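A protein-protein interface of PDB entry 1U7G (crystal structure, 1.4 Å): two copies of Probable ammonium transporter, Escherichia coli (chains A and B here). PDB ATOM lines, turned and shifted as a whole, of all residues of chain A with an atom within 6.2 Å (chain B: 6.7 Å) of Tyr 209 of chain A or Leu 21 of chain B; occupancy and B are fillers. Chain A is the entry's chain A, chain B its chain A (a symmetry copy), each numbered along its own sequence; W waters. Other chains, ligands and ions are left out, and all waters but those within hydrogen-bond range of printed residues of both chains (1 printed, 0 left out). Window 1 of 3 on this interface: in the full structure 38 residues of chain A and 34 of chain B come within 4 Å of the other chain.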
ATOM      1  N   MET A  23      13.366 -27.233  15.891  1.00  0.00           N
ATOM      2  CA  MET A  23      14.765 -27.297  15.433  1.00  0.00           C
ATOM      3  C   MET A  23      15.229 -28.739  15.379  1.00  0.00           C
ATOM      4  O   MET A  23      16.054 -29.068  14.528  1.00  0.00           O
ATOM      5  CB  MET A  23      15.713 -26.558  16.405  1.00  0.00           C
ATOM      6  CG  MET A  23      15.407 -25.054  16.439  1.00  0.00           C
ATOM      7  SD  MET A  23      16.491 -24.208  17.690  1.00  0.00           S
ATOM      8  CE  MET A  23      18.037 -24.319  16.667  1.00  0.00           C
ATOM      9  N   GLY A 204      16.282 -27.902   6.111  1.00  0.00           N
ATOM     10  CA  GLY A 204      16.639 -28.051   7.516  1.00  0.00           C
ATOM     11  C   GLY A 204      17.260 -26.783   8.078  1.00  0.00           C
ATOM     12  O   GLY A 204      16.967 -26.395   9.238  1.00  0.00           O
ATOM     13  N   THR A 205      18.117 -26.152   7.281  1.00  0.00           N
ATOM     14  CA  THR A 205      18.705 -24.880   7.764  1.00  0.00           C
ATOM     15  C   THR A 205      17.588 -23.897   8.037  1.00  0.00           C
ATOM     16  O   THR A 205      17.642 -23.175   9.057  1.00  0.00           O
ATOM     17  CB  THR A 205      19.615 -24.283   6.668  1.00  0.00           C
ATOM     18  OG1 THR A 205      20.675 -25.265   6.448  1.00  0.00           O
ATOM     19  CG2 THR A 205      20.281 -22.990   7.076  1.00  0.00           C
ATOM     20  N   ALA A 206      16.590 -23.831   7.151  1.00  0.00           N
ATOM     21  CA  ALA A 206      15.520 -22.845   7.312  1.00  0.00           C
ATOM     22  C   ALA A 206      14.753 -23.123   8.591  1.00  0.00           C
ATOM     23  O   ALA A 206      14.416 -22.186   9.304  1.00  0.00           O
ATOM     24  CB  ALA A 206      14.579 -22.921   6.125  1.00  0.00           C
ATOM     25  N   ILE A 207      14.452 -24.370   8.858  1.00  0.00           N
ATOM     26  CA  ILE A 207      13.695 -24.696  10.045  1.00  0.00           C
ATOM     27  C   ILE A 207      14.549 -24.414  11.273  1.00  0.00           C
ATOM     28  O   ILE A 207      14.039 -23.922  12.279  1.00  0.00           O
ATOM     29  CB  ILE A 207      13.271 -26.150   9.996  1.00  0.00           C
ATOM     30  CG1 ILE A 207      12.196 -26.308   8.910  1.00  0.00           C
ATOM     31  CG2 ILE A 207      12.736 -26.648  11.357  1.00  0.00           C
ATOM     32  CD1 ILE A 207      11.831 -27.790   8.693  1.00  0.00           C
ATOM     33  N   LEU A 208      15.842 -24.743  11.253  1.00  0.00           N
ATOM     34  CA  LEU A 208      16.756 -24.402  12.339  1.00  0.00           C
ATOM     35  C   LEU A 208      16.723 -22.896  12.527  1.00  0.00           C
ATOM     36  O   LEU A 208      16.699 -22.445  13.662  1.00  0.00           O
ATOM     37  CB  LEU A 208      18.198 -24.827  12.048  1.00  0.00           C
ATOM     38  CG  LEU A 208      18.383 -26.348  12.151  1.00  0.00           C
ATOM     39  CD1 LEU A 208      19.664 -26.775  11.452  1.00  0.00           C
ATOM     40  CD2 LEU A 208      18.404 -26.780  13.609  1.00  0.00           C
ATOM     41  N   TYR A 209      16.766 -22.128  11.450  1.00  0.00           N
ATOM     42  CA  TYR A 209      16.764 -20.658  11.600  1.00  0.00           C
ATOM     43  C   TYR A 209      15.477 -20.169  12.258  1.00  0.00           C
ATOM     44  O   TYR A 209      15.538 -19.371  13.203  1.00  0.00           O
ATOM     45  CB  TYR A 209      16.870 -20.092  10.200  1.00  0.00           C
ATOM     46  CG  TYR A 209      16.696 -18.584  10.078  1.00  0.00           C
ATOM     47  CD1 TYR A 209      17.653 -17.740  10.629  1.00  0.00           C
ATOM     48  CD2 TYR A 209      15.573 -18.074   9.451  1.00  0.00           C
ATOM     49  CE1 TYR A 209      17.436 -16.364  10.500  1.00  0.00           C
ATOM     50  CE2 TYR A 209      15.367 -16.707   9.305  1.00  0.00           C
ATOM     51  CZ  TYR A 209      16.342 -15.864   9.853  1.00  0.00           C
ATOM     52  OH  TYR A 209      16.161 -14.506   9.726  1.00  0.00           O
ATOM     53  N   ILE A 210      14.337 -20.630  11.758  1.00  0.00           N
ATOM     54  CA  ILE A 210      13.104 -20.095  12.354  1.00  0.00           C
ATOM     55  C   ILE A 210      12.978 -20.572  13.801  1.00  0.00           C
ATOM     56  O   ILE A 210      12.580 -19.783  14.663  1.00  0.00           O
ATOM     57  CB  ILE A 210      11.919 -20.596  11.507  1.00  0.00           C
ATOM     58  CG1 ILE A 210      12.028 -20.044  10.064  1.00  0.00           C
ATOM     59  CG2 ILE A 210      10.580 -20.271  12.163  1.00  0.00           C
ATOM     60  CD1 ILE A 210      12.029 -18.498  10.046  1.00  0.00           C
ATOM     61  N   GLY A 211      13.365 -21.829  14.056  1.00  0.00           N
ATOM     62  CA  GLY A 211      13.241 -22.291  15.458  1.00  0.00           C
ATOM     63  C   GLY A 211      14.214 -21.524  16.322  1.00  0.00           C
ATOM     64  O   GLY A 211      13.931 -21.363  17.514  1.00  0.00           O
ATOM     65  N   TRP A 212      15.319 -21.053  15.698  1.00  0.00           N
ATOM     66  CA  TRP A 212      16.323 -20.422  16.535  1.00  0.00           C
ATOM     67  C   TRP A 212      15.835 -19.084  17.126  1.00  0.00           C
ATOM     68  O   TRP A 212      16.487 -18.606  18.058  1.00  0.00           O
ATOM     69  CB  TRP A 212      17.540 -20.148  15.676  1.00  0.00           C
ATOM     70  CG  TRP A 212      18.856 -20.320  16.336  1.00  0.00           C
ATOM     71  CD1 TRP A 212      19.354 -19.652  17.430  1.00  0.00           C
ATOM     72  CD2 TRP A 212      19.891 -21.231  15.914  1.00  0.00           C
ATOM     73  NE1 TRP A 212      20.628 -20.110  17.705  1.00  0.00           N
ATOM     74  CE2 TRP A 212      20.977 -21.070  16.794  1.00  0.00           C
ATOM     75  CE3 TRP A 212      19.931 -22.140  14.868  1.00  0.00           C
ATOM     76  CZ2 TRP A 212      22.155 -21.822  16.643  1.00  0.00           C
ATOM     77  CZ3 TRP A 212      21.110 -22.896  14.719  1.00  0.00           C
ATOM     78  CH2 TRP A 212      22.181 -22.722  15.612  1.00  0.00           C
ATOM     79  N   PHE A 213      14.762 -18.554  16.538  1.00  0.00           N
ATOM     80  CA  PHE A 213      14.203 -17.371  17.200  1.00  0.00           C
ATOM     81  C   PHE A 213      13.674 -17.787  18.557  1.00  0.00           C
ATOM     82  O   PHE A 213      13.775 -17.024  19.525  1.00  0.00           O
ATOM     83  CB  PHE A 213      13.108 -16.723  16.354  1.00  0.00           C
ATOM     84  CG  PHE A 213      13.828 -16.061  15.178  1.00  0.00           C
ATOM     85  CD1 PHE A 213      14.485 -14.842  15.338  1.00  0.00           C
ATOM     86  CD2 PHE A 213      13.854 -16.682  13.930  1.00  0.00           C
ATOM     87  CE1 PHE A 213      15.162 -14.233  14.272  1.00  0.00           C
ATOM     88  CE2 PHE A 213      14.538 -16.112  12.855  1.00  0.00           C
ATOM     89  CZ  PHE A 213      15.197 -14.890  13.047  1.00  0.00           C
ATOM     90  N   GLY A 214      13.080 -18.978  18.665  1.00  0.00           N
ATOM     91  CA  GLY A 214      12.576 -19.436  19.971  1.00  0.00           C
ATOM     92  C   GLY A 214      13.767 -19.650  20.882  1.00  0.00           C
ATOM     93  O   GLY A 214      13.742 -19.362  22.089  1.00  0.00           O
ATOM     94  N   PHE A 231      16.100 -11.213  19.264  1.00  0.00           N
ATOM     95  CA  PHE A 231      15.437 -11.538  17.988  1.00  0.00           C
ATOM     96  C   PHE A 231      16.136 -10.774  16.882  1.00  0.00           C
ATOM     97  O   PHE A 231      16.496 -11.366  15.856  1.00  0.00           O
ATOM     98  CB  PHE A 231      13.969 -11.141  18.107  1.00  0.00           C
ATOM     99  CG  PHE A 231      13.096 -11.751  17.013  1.00  0.00           C
ATOM    100  CD1 PHE A 231      13.196 -11.365  15.688  1.00  0.00           C
ATOM    101  CD2 PHE A 231      12.191 -12.761  17.374  1.00  0.00           C
ATOM    102  CE1 PHE A 231      12.458 -11.915  14.675  1.00  0.00           C
ATOM    103  CE2 PHE A 231      11.423 -13.310  16.364  1.00  0.00           C
ATOM    104  CZ  PHE A 231      11.588 -12.924  15.050  1.00  0.00           C
ATOM    105  N   THR A 234      19.511 -11.958  16.087  1.00  0.00           N
ATOM    106  CA  THR A 234      19.523 -13.258  15.392  1.00  0.00           C
ATOM    107  C   THR A 234      19.315 -13.013  13.916  1.00  0.00           C
ATOM    108  O   THR A 234      20.000 -13.589  13.067  1.00  0.00           O
ATOM    109  CB  THR A 234      18.408 -14.139  15.946  1.00  0.00           C
ATOM    110  OG1 THR A 234      18.723 -14.389  17.326  1.00  0.00           O
ATOM    111  CG2 THR A 234      18.376 -15.485  15.253  1.00  0.00           C
ATOM    112  N   VAL A 235      18.390 -12.137  13.557  1.00  0.00           N
ATOM    113  CA  VAL A 235      18.168 -11.832  12.152  1.00  0.00           C
ATOM    114  C   VAL A 235      19.471 -11.312  11.536  1.00  0.00           C
ATOM    115  O   VAL A 235      19.950 -11.692  10.461  1.00  0.00           O
ATOM    116  CB  VAL A 235      17.075 -10.762  11.964  1.00  0.00           C
ATOM    117  CG1 VAL A 235      17.024 -10.299  10.498  1.00  0.00           C
ATOM    118  CG2 VAL A 235      15.717 -11.337  12.435  1.00  0.00           C
ATOM    119  N   THR A 238      22.634 -13.675  11.557  1.00  0.00           N
ATOM    120  CA  THR A 238      22.539 -14.756  10.577  1.00  0.00           C
ATOM    121  C   THR A 238      22.785 -14.231   9.168  1.00  0.00           C
ATOM    122  O   THR A 238      23.517 -14.802   8.355  1.00  0.00           O
ATOM    123  CB  THR A 238      21.120 -15.351  10.584  1.00  0.00           C
ATOM    124  OG1 THR A 238      20.890 -15.871  11.906  1.00  0.00           O
ATOM    125  CG2 THR A 238      21.051 -16.513   9.608  1.00  0.00           C
ATOM    126  N   ALA A 239      22.185 -13.099   8.860  1.00  0.00           N
ATOM    127  CA  ALA A 239      22.294 -12.490   7.534  1.00  0.00           C
ATOM    128  C   ALA A 239      23.732 -12.105   7.286  1.00  0.00           C
ATOM    129  O   ALA A 239      24.257 -12.296   6.198  1.00  0.00           O
ATOM    130  CB  ALA A 239      21.385 -11.277   7.508  1.00  0.00           C
ATOM    131  N   ALA A 265      24.547 -19.307   7.357  1.00  0.00           N
ATOM    132  CA  ALA A 265      23.388 -19.063   8.233  1.00  0.00           C
ATOM    133  C   ALA A 265      23.651 -19.720   9.573  1.00  0.00           C
ATOM    134  O   ALA A 265      23.519 -19.063  10.621  1.00  0.00           O
ATOM    135  CB  ALA A 265      22.089 -19.610   7.620  1.00  0.00           C
ATOM    136  N   ILE A 266      24.056 -21.007   9.542  1.00  0.00           N
ATOM    137  CA  ILE A 266      24.284 -21.688  10.808  1.00  0.00           C
ATOM    138  C   ILE A 266      25.403 -20.986  11.593  1.00  0.00           C
ATOM    139  O   ILE A 266      25.377 -20.870  12.801  1.00  0.00           O
ATOM    140  CB  ILE A 266      24.591 -23.185  10.540  1.00  0.00           C
ATOM    141  CG1 ILE A 266      23.455 -23.902   9.835  1.00  0.00           C
ATOM    142  CG2 ILE A 266      24.964 -23.882  11.841  1.00  0.00           C
ATOM    143  CD1 ILE A 266      22.112 -23.884  10.614  1.00  0.00           C
ATOM    144  N   LEU A 269      24.074 -17.987  13.287  1.00  0.00           N
ATOM    145  CA  LEU A 269      23.170 -18.403  14.369  1.00  0.00           C
ATOM    146  C   LEU A 269      23.951 -18.925  15.555  1.00  0.00           C
ATOM    147  O   LEU A 269      23.676 -18.544  16.698  1.00  0.00           O
ATOM    148  CB  LEU A 269      22.225 -19.503  13.853  1.00  0.00           C
ATOM    149  CG  LEU A 269      21.179 -18.925  12.886  1.00  0.00           C
ATOM    150  CD1 LEU A 269      20.619 -20.037  12.027  1.00  0.00           C
ATOM    151  CD2 LEU A 269      20.092 -18.187  13.648  1.00  0.00           C
ATOM    152  N   CYS B  16       4.855 -13.530  15.229  1.00  0.00           N
ATOM    153  CA  CYS B  16       4.379 -13.220  13.878  1.00  0.00           C
ATOM    154  C   CYS B  16       5.589 -12.909  13.004  1.00  0.00           C
ATOM    155  O   CYS B  16       5.562 -13.253  11.826  1.00  0.00           O
ATOM    156  CB  CYS B  16       3.423 -12.016  13.837  1.00  0.00           C
ATOM    157  SG  CYS B  16       1.809 -12.415  14.499  1.00  0.00           S
ATOM    158  N   THR B  17       6.599 -12.227  13.522  1.00  0.00           N
ATOM    159  CA  THR B  17       7.769 -11.970  12.670  1.00  0.00           C
ATOM    160  C   THR B  17       8.464 -13.274  12.295  1.00  0.00           C
ATOM    161  O   THR B  17       8.823 -13.392  11.129  1.00  0.00           O
ATOM    162  CB  THR B  17       8.778 -11.108  13.447  1.00  0.00           C
ATOM    163  OG1 THR B  17       8.164  -9.865  13.820  1.00  0.00           O
ATOM    164  CG2 THR B  17       9.964 -10.750  12.574  1.00  0.00           C
ATOM    165  N   ALA B  18       8.598 -14.197  13.263  1.00  0.00           N
ATOM    166  CA  ALA B  18       9.180 -15.495  12.916  1.00  0.00           C
ATOM    167  C   ALA B  18       8.342 -16.146  11.829  1.00  0.00           C
ATOM    168  O   ALA B  18       8.906 -16.717  10.890  1.00  0.00           O
ATOM    169  CB  ALA B  18       9.259 -16.368  14.156  1.00  0.00           C
ATOM    170  N   LEU B  19       7.044 -16.073  11.932  1.00  0.00           N
ATOM    171  CA  LEU B  19       6.179 -16.658  10.902  1.00  0.00           C
ATOM    172  C   LEU B  19       6.402 -15.979   9.581  1.00  0.00           C
ATOM    173  O   LEU B  19       6.391 -16.649   8.541  1.00  0.00           O
ATOM    174  CB  LEU B  19       4.730 -16.504  11.313  1.00  0.00           C
ATOM    175  CG  LEU B  19       4.331 -17.489  12.408  1.00  0.00           C
ATOM    176  CD1 LEU B  19       2.927 -17.129  12.914  1.00  0.00           C
ATOM    177  CD2 LEU B  19       4.349 -18.912  11.864  1.00  0.00           C
ATOM    178  N   VAL B  20       6.559 -14.657   9.582  1.00  0.00           N
ATOM    179  CA  VAL B  20       6.777 -14.010   8.256  1.00  0.00           C
ATOM    180  C   VAL B  20       8.139 -14.430   7.699  1.00  0.00           C
ATOM    181  O   VAL B  20       8.284 -14.650   6.484  1.00  0.00           O
ATOM    182  CB  VAL B  20       6.653 -12.493   8.310  1.00  0.00           C
ATOM    183  CG1 VAL B  20       6.924 -11.843   6.954  1.00  0.00           C
ATOM    184  CG2 VAL B  20       5.209 -12.149   8.746  1.00  0.00           C
ATOM    185  N   LEU B  21       9.154 -14.505   8.563  1.00  0.00           N
ATOM    186  CA  LEU B  21      10.482 -14.944   8.069  1.00  0.00           C
ATOM    187  C   LEU B  21      10.357 -16.340   7.478  1.00  0.00           C
ATOM    188  O   LEU B  21      11.000 -16.645   6.493  1.00  0.00           O
ATOM    189  CB  LEU B  21      11.488 -14.907   9.202  1.00  0.00           C
ATOM    190  CG  LEU B  21      11.790 -13.496   9.677  1.00  0.00           C
ATOM    191  CD1 LEU B  21      12.677 -13.513  10.917  1.00  0.00           C
ATOM    192  CD2 LEU B  21      12.499 -12.678   8.579  1.00  0.00           C
ATOM    193  N   PHE B  22       9.538 -17.176   8.093  1.00  0.00           N
ATOM    194  CA  PHE B  22       9.316 -18.560   7.649  1.00  0.00           C
ATOM    195  C   PHE B  22       8.762 -18.532   6.240  1.00  0.00           C
ATOM    196  O   PHE B  22       9.016 -19.500   5.499  1.00  0.00           O
ATOM    197  CB  PHE B  22       8.366 -19.192   8.653  1.00  0.00           C
ATOM    198  CG  PHE B  22       8.064 -20.660   8.574  1.00  0.00           C
ATOM    199  CD1 PHE B  22       9.040 -21.592   8.297  1.00  0.00           C
ATOM    200  CD2 PHE B  22       6.760 -21.087   8.827  1.00  0.00           C
ATOM    201  CE1 PHE B  22       8.765 -22.946   8.282  1.00  0.00           C
ATOM    202  CE2 PHE B  22       6.467 -22.435   8.867  1.00  0.00           C
ATOM    203  CZ  PHE B  22       7.492 -23.350   8.648  1.00  0.00           C
ATOM    204  N   MET B  23       7.969 -17.550   5.888  1.00  0.00           N
ATOM    205  CA  MET B  23       7.426 -17.452   4.522  1.00  0.00           C
ATOM    206  C   MET B  23       8.557 -17.388   3.517  1.00  0.00           C
ATOM    207  O   MET B  23       8.393 -17.881   2.401  1.00  0.00           O
ATOM    208  CB  MET B  23       6.589 -16.165   4.336  1.00  0.00           C
ATOM    209  CG  MET B  23       5.338 -16.187   5.228  1.00  0.00           C
ATOM    210  SD  MET B  23       4.408 -14.586   5.060  1.00  0.00           S
ATOM    211  CE  MET B  23       3.746 -14.959   3.365  1.00  0.00           C
ATOM    212  N   THR B  24       9.669 -16.741   3.835  1.00  0.00           N
ATOM    213  CA  THR B  24      10.756 -16.706   2.861  1.00  0.00           C
ATOM    214  C   THR B  24      11.647 -17.930   3.000  1.00  0.00           C
ATOM    215  O   THR B  24      11.975 -18.597   2.037  1.00  0.00           O
ATOM    216  CB  THR B  24      11.597 -15.418   3.085  1.00  0.00           C
ATOM    217  OG1 THR B  24      10.727 -14.276   2.945  1.00  0.00           O
ATOM    218  CG2 THR B  24      12.686 -15.355   2.037  1.00  0.00           C
ATOM    219  N   ILE B  25      12.024 -18.129   4.270  1.00  0.00           N
ATOM    220  CA  ILE B  25      13.006 -19.132   4.643  1.00  0.00           C
ATOM    221  C   ILE B  25      12.264 -20.192   5.427  1.00  0.00           C
ATOM    222  O   ILE B  25      12.134 -20.076   6.650  1.00  0.00           O
ATOM    223  CB  ILE B  25      14.114 -18.491   5.474  1.00  0.00           C
ATOM    224  CG1 ILE B  25      14.800 -17.391   4.675  1.00  0.00           C
ATOM    225  CG2 ILE B  25      15.097 -19.554   5.942  1.00  0.00           C
ATOM    226  CD1 ILE B  25      15.483 -17.904   3.388  1.00  0.00           C
ATOM    227  N   PRO B  26      11.731 -21.278   4.869  1.00  0.00           N
ATOM    228  CA  PRO B  26      11.947 -21.647   3.469  1.00  0.00           C
ATOM    229  C   PRO B  26      10.744 -21.576   2.554  1.00  0.00           C
ATOM    230  O   PRO B  26      10.863 -22.046   1.440  1.00  0.00           O
ATOM    231  CB  PRO B  26      12.252 -23.151   3.675  1.00  0.00           C
ATOM    232  CG  PRO B  26      11.255 -23.567   4.708  1.00  0.00           C
ATOM    233  CD  PRO B  26      11.054 -22.353   5.615  1.00  0.00           C
ATOM    234  N   GLY B  27       9.642 -20.980   2.998  1.00  0.00           N
ATOM    235  CA  GLY B  27       8.356 -21.053   2.257  1.00  0.00           C
ATOM    236  C   GLY B  27       8.520 -20.752   0.776  1.00  0.00           C
ATOM    237  O   GLY B  27       8.221 -21.620  -0.069  1.00  0.00           O
ATOM    238  N   PHE B  52      18.050 -12.772   0.753  1.00  0.00           N
ATOM    239  CA  PHE B  52      17.354 -12.649   2.064  1.00  0.00           C
ATOM    240  C   PHE B  52      18.297 -11.980   3.053  1.00  0.00           C
ATOM    241  O   PHE B  52      17.957 -11.040   3.759  1.00  0.00           O
ATOM    242  CB  PHE B  52      16.910 -14.045   2.490  1.00  0.00           C
ATOM    243  CG  PHE B  52      16.453 -14.079   3.952  1.00  0.00           C
ATOM    244  CD1 PHE B  52      15.162 -13.653   4.252  1.00  0.00           C
ATOM    245  CD2 PHE B  52      17.286 -14.523   4.967  1.00  0.00           C
ATOM    246  CE1 PHE B  52      14.709 -13.710   5.572  1.00  0.00           C
ATOM    247  CE2 PHE B  52      16.821 -14.567   6.272  1.00  0.00           C
ATOM    248  CZ  PHE B  52      15.530 -14.146   6.581  1.00  0.00           C
ATOM    249  N   CYS B  56      17.938  -8.374   4.891  1.00  0.00           N
ATOM    250  CA  CYS B  56      17.983  -8.253   6.336  1.00  0.00           C
ATOM    251  C   CYS B  56      18.975  -7.191   6.772  1.00  0.00           C
ATOM    252  O   CYS B  56      18.668  -6.413   7.694  1.00  0.00           O
ATOM    253  CB  CYS B  56      18.411  -9.540   7.032  1.00  0.00           C
ATOM    254  SG  CYS B  56      17.102 -10.812   6.932  1.00  0.00           S
ATOM    255  N   ALA B 102      11.929  -5.606  13.246  1.00  0.00           N
ATOM    256  CA  ALA B 102      12.077  -6.982  12.734  1.00  0.00           C
ATOM    257  C   ALA B 102      10.871  -7.383  11.923  1.00  0.00           C
ATOM    258  O   ALA B 102      10.997  -7.990  10.860  1.00  0.00           O
ATOM    259  CB  ALA B 102      12.278  -8.007  13.868  1.00  0.00           C
ATOM    260  N   GLY B 105      10.993  -5.730   8.712  1.00  0.00           N
ATOM    261  CA  GLY B 105      12.062  -6.262   7.852  1.00  0.00           C
ATOM    262  C   GLY B 105      11.615  -7.554   7.223  1.00  0.00           C
ATOM    263  O   GLY B 105      11.975  -7.853   6.067  1.00  0.00           O
ATOM    264  N   SER B 106      10.815  -8.316   7.968  1.00  0.00           N
ATOM    265  CA  SER B 106      10.421  -9.618   7.442  1.00  0.00           C
ATOM    266  C   SER B 106       9.561  -9.455   6.202  1.00  0.00           C
ATOM    267  O   SER B 106       9.537 -10.294   5.310  1.00  0.00           O
ATOM    268  CB  SER B 106       9.777 -10.484   8.520  1.00  0.00           C
ATOM    269  OG  SER B 106       8.496  -9.978   8.887  1.00  0.00           O
ATOM    270  N   PHE B 107       8.837  -8.354   6.135  1.00  0.00           N
ATOM    271  CA  PHE B 107       8.001  -8.103   4.974  1.00  0.00           C
ATOM    272  C   PHE B 107       8.873  -7.770   3.785  1.00  0.00           C
ATOM    273  O   PHE B 107       8.578  -8.147   2.655  1.00  0.00           O
ATOM    274  CB  PHE B 107       7.059  -6.906   5.212  1.00  0.00           C
ATOM    275  CG  PHE B 107       5.776  -7.319   5.873  1.00  0.00           C
ATOM    276  CD1 PHE B 107       5.783  -7.972   7.107  1.00  0.00           C
ATOM    277  CD2 PHE B 107       4.577  -7.058   5.238  1.00  0.00           C
ATOM    278  CE1 PHE B 107       4.623  -8.394   7.712  1.00  0.00           C
ATOM    279  CE2 PHE B 107       3.398  -7.482   5.880  1.00  0.00           C
ATOM    280  CZ  PHE B 107       3.419  -8.107   7.119  1.00  0.00           C
ATOM    281  N   CYS B 109      11.690  -8.927   3.285  1.00  0.00           N
ATOM    282  CA  CYS B 109      12.316 -10.173   2.862  1.00  0.00           C
ATOM    283  C   CYS B 109      11.369 -10.980   2.002  1.00  0.00           C
ATOM    284  O   CYS B 109      11.783 -11.497   0.955  1.00  0.00           O
ATOM    285  CB  CYS B 109      12.694 -11.031   4.083  1.00  0.00           C
ATOM    286  SG  CYS B 109      14.101 -10.284   4.963  1.00  0.00           S
ATOM    287  N   ILE B 110      10.104 -11.119   2.438  1.00  0.00           N
ATOM    288  CA  ILE B 110       9.263 -12.030   1.614  1.00  0.00           C
ATOM    289  C   ILE B 110       9.016 -11.318   0.298  1.00  0.00           C
ATOM    290  O   ILE B 110       8.888 -11.941  -0.766  1.00  0.00           O
ATOM    291  CB  ILE B 110       7.978 -12.429   2.325  1.00  0.00           C
ATOM    292  CG1 ILE B 110       7.093 -13.330   1.439  1.00  0.00           C
ATOM    293  CG2 ILE B 110       7.160 -11.213   2.795  1.00  0.00           C
ATOM    294  CD1 ILE B 110       7.774 -14.625   1.026  1.00  0.00           C
ATOM    295  N   GLY B 211       2.700 -19.024   7.515  1.00  0.00           N
ATOM    296  CA  GLY B 211       3.433 -17.792   7.888  1.00  0.00           C
ATOM    297  C   GLY B 211       2.541 -16.595   7.657  1.00  0.00           C
ATOM    298  O   GLY B 211       2.724 -15.591   8.353  1.00  0.00           O
HETATM  299  O   HOH W   1      18.382 -13.240   8.898  1.00  0.00           O
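Hydrophobic or aromatic side chains of chain B within 4 Å of the printed part of chain A: Leu 21, Phe 22, Ile 25, Pro 26, Phe 52 and Ala 102.
Printed residues of chain A that touch a printed residue of chain B: Ala 206, Tyr 209, Ile 210, Phe 213, Phe 231, Val 235 and Ala 239.
Hydrophobic or aromatic side chains of chain A within 4 Å of the printed part of chain B: Ala 206, Tyr 209, Ile 210, Phe 213, Phe 231, Val 235 and Ala 239.
Among the printed residues, 15 pairs touch across the chains.
O of Phe 22 of chain B lies within hydrogen-bond range of N of Gly 27 of chain B (3.0 Å).
O of Phe 52 of chain B sits at hydrogen-bond distance from SG of Cys 56 of chain B (3.3 Å).
The side-chain sulfur (SG) of Cys 56 of chain B sits at hydrogen-bond distance from the side-chain sulfur (SG) of Cys 109 of chain B, at 3.6 Å.
Among the printed residues, merely in contact across the chains: Tyr 209 of chain A with Phe 52 of chain B (3.2 Å), Ala 206 of chain A with Pro 26 of chain B (3.4 Å), Ala 206 of chain A with Ile 25 of chain B (3.4 Å), Ile 210 of chain A with Ile 25 of chain B (3.4 Å), Ile 210 of chain A with Phe 22 of chain B (3.4 Å), Phe 231 of chain A with Thr 17 of chain B (3.5 Å), Ala 239 of chain A with Cys 56 of chain B (3.5 Å), Phe 213 of chain A with Leu 21 of chain B (3.6 Å), Val 235 of chain A with Cys 56 of chain B (3.6 Å), Ile 210 of chain A with Ala 18 of chain B (3.7 Å), Phe 231 of chain A with Ala 18 of chain B (3.7 Å), Ile 210 of chain A with Leu 21 of chain B (3.7 Å), Tyr 209 of chain A with Leu 21 of chain B (3.8 Å), Tyr 209 of chain A with Ile 25 of chain B (3.8 Å) and Phe 231 of chain A with Ala 102 of chain B (3.9 Å).
2 positions are printed for both chains.
Water W1 lies within hydrogen-bond range of OH of Tyr 209 of chain A (2.7 Å), O of Val 235 of chain A (2.7 Å) and SG of Cys 56 of chain B (3.4 Å).
Tyr 209 of chain A touches just these residues of chain B: Leu 21 (3.8 Å), Ile 25 (3.8 Å) and Phe 52 (3.2 Å).
Printed residues of chain A within 4 Å of Ile 25 of chain B: Ala 206, Tyr 209 and Ile 210.
Of the printed residues of chain A, Cys 56 of chain B touches Val 235 and Ala 239.
Of the printed residues of chain A, Ala 102 of chain B touches Phe 231.
Printed residues of chain A within 4 Å of Phe 52 of chain B: Tyr 209.
Cys 16 of chain B touches none of the printed residues of chain A.
Leu 19 of chain B touches none of the printed residues of chain A.
The nearest residue of chain A that does not touch Leu 21 of chain B is Val 235 of chain A (4.03 Å).
The nearest printed residue of chain B that does not touch Ala 239 of chain A is Phe 52 of chain B (5.1 Å).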
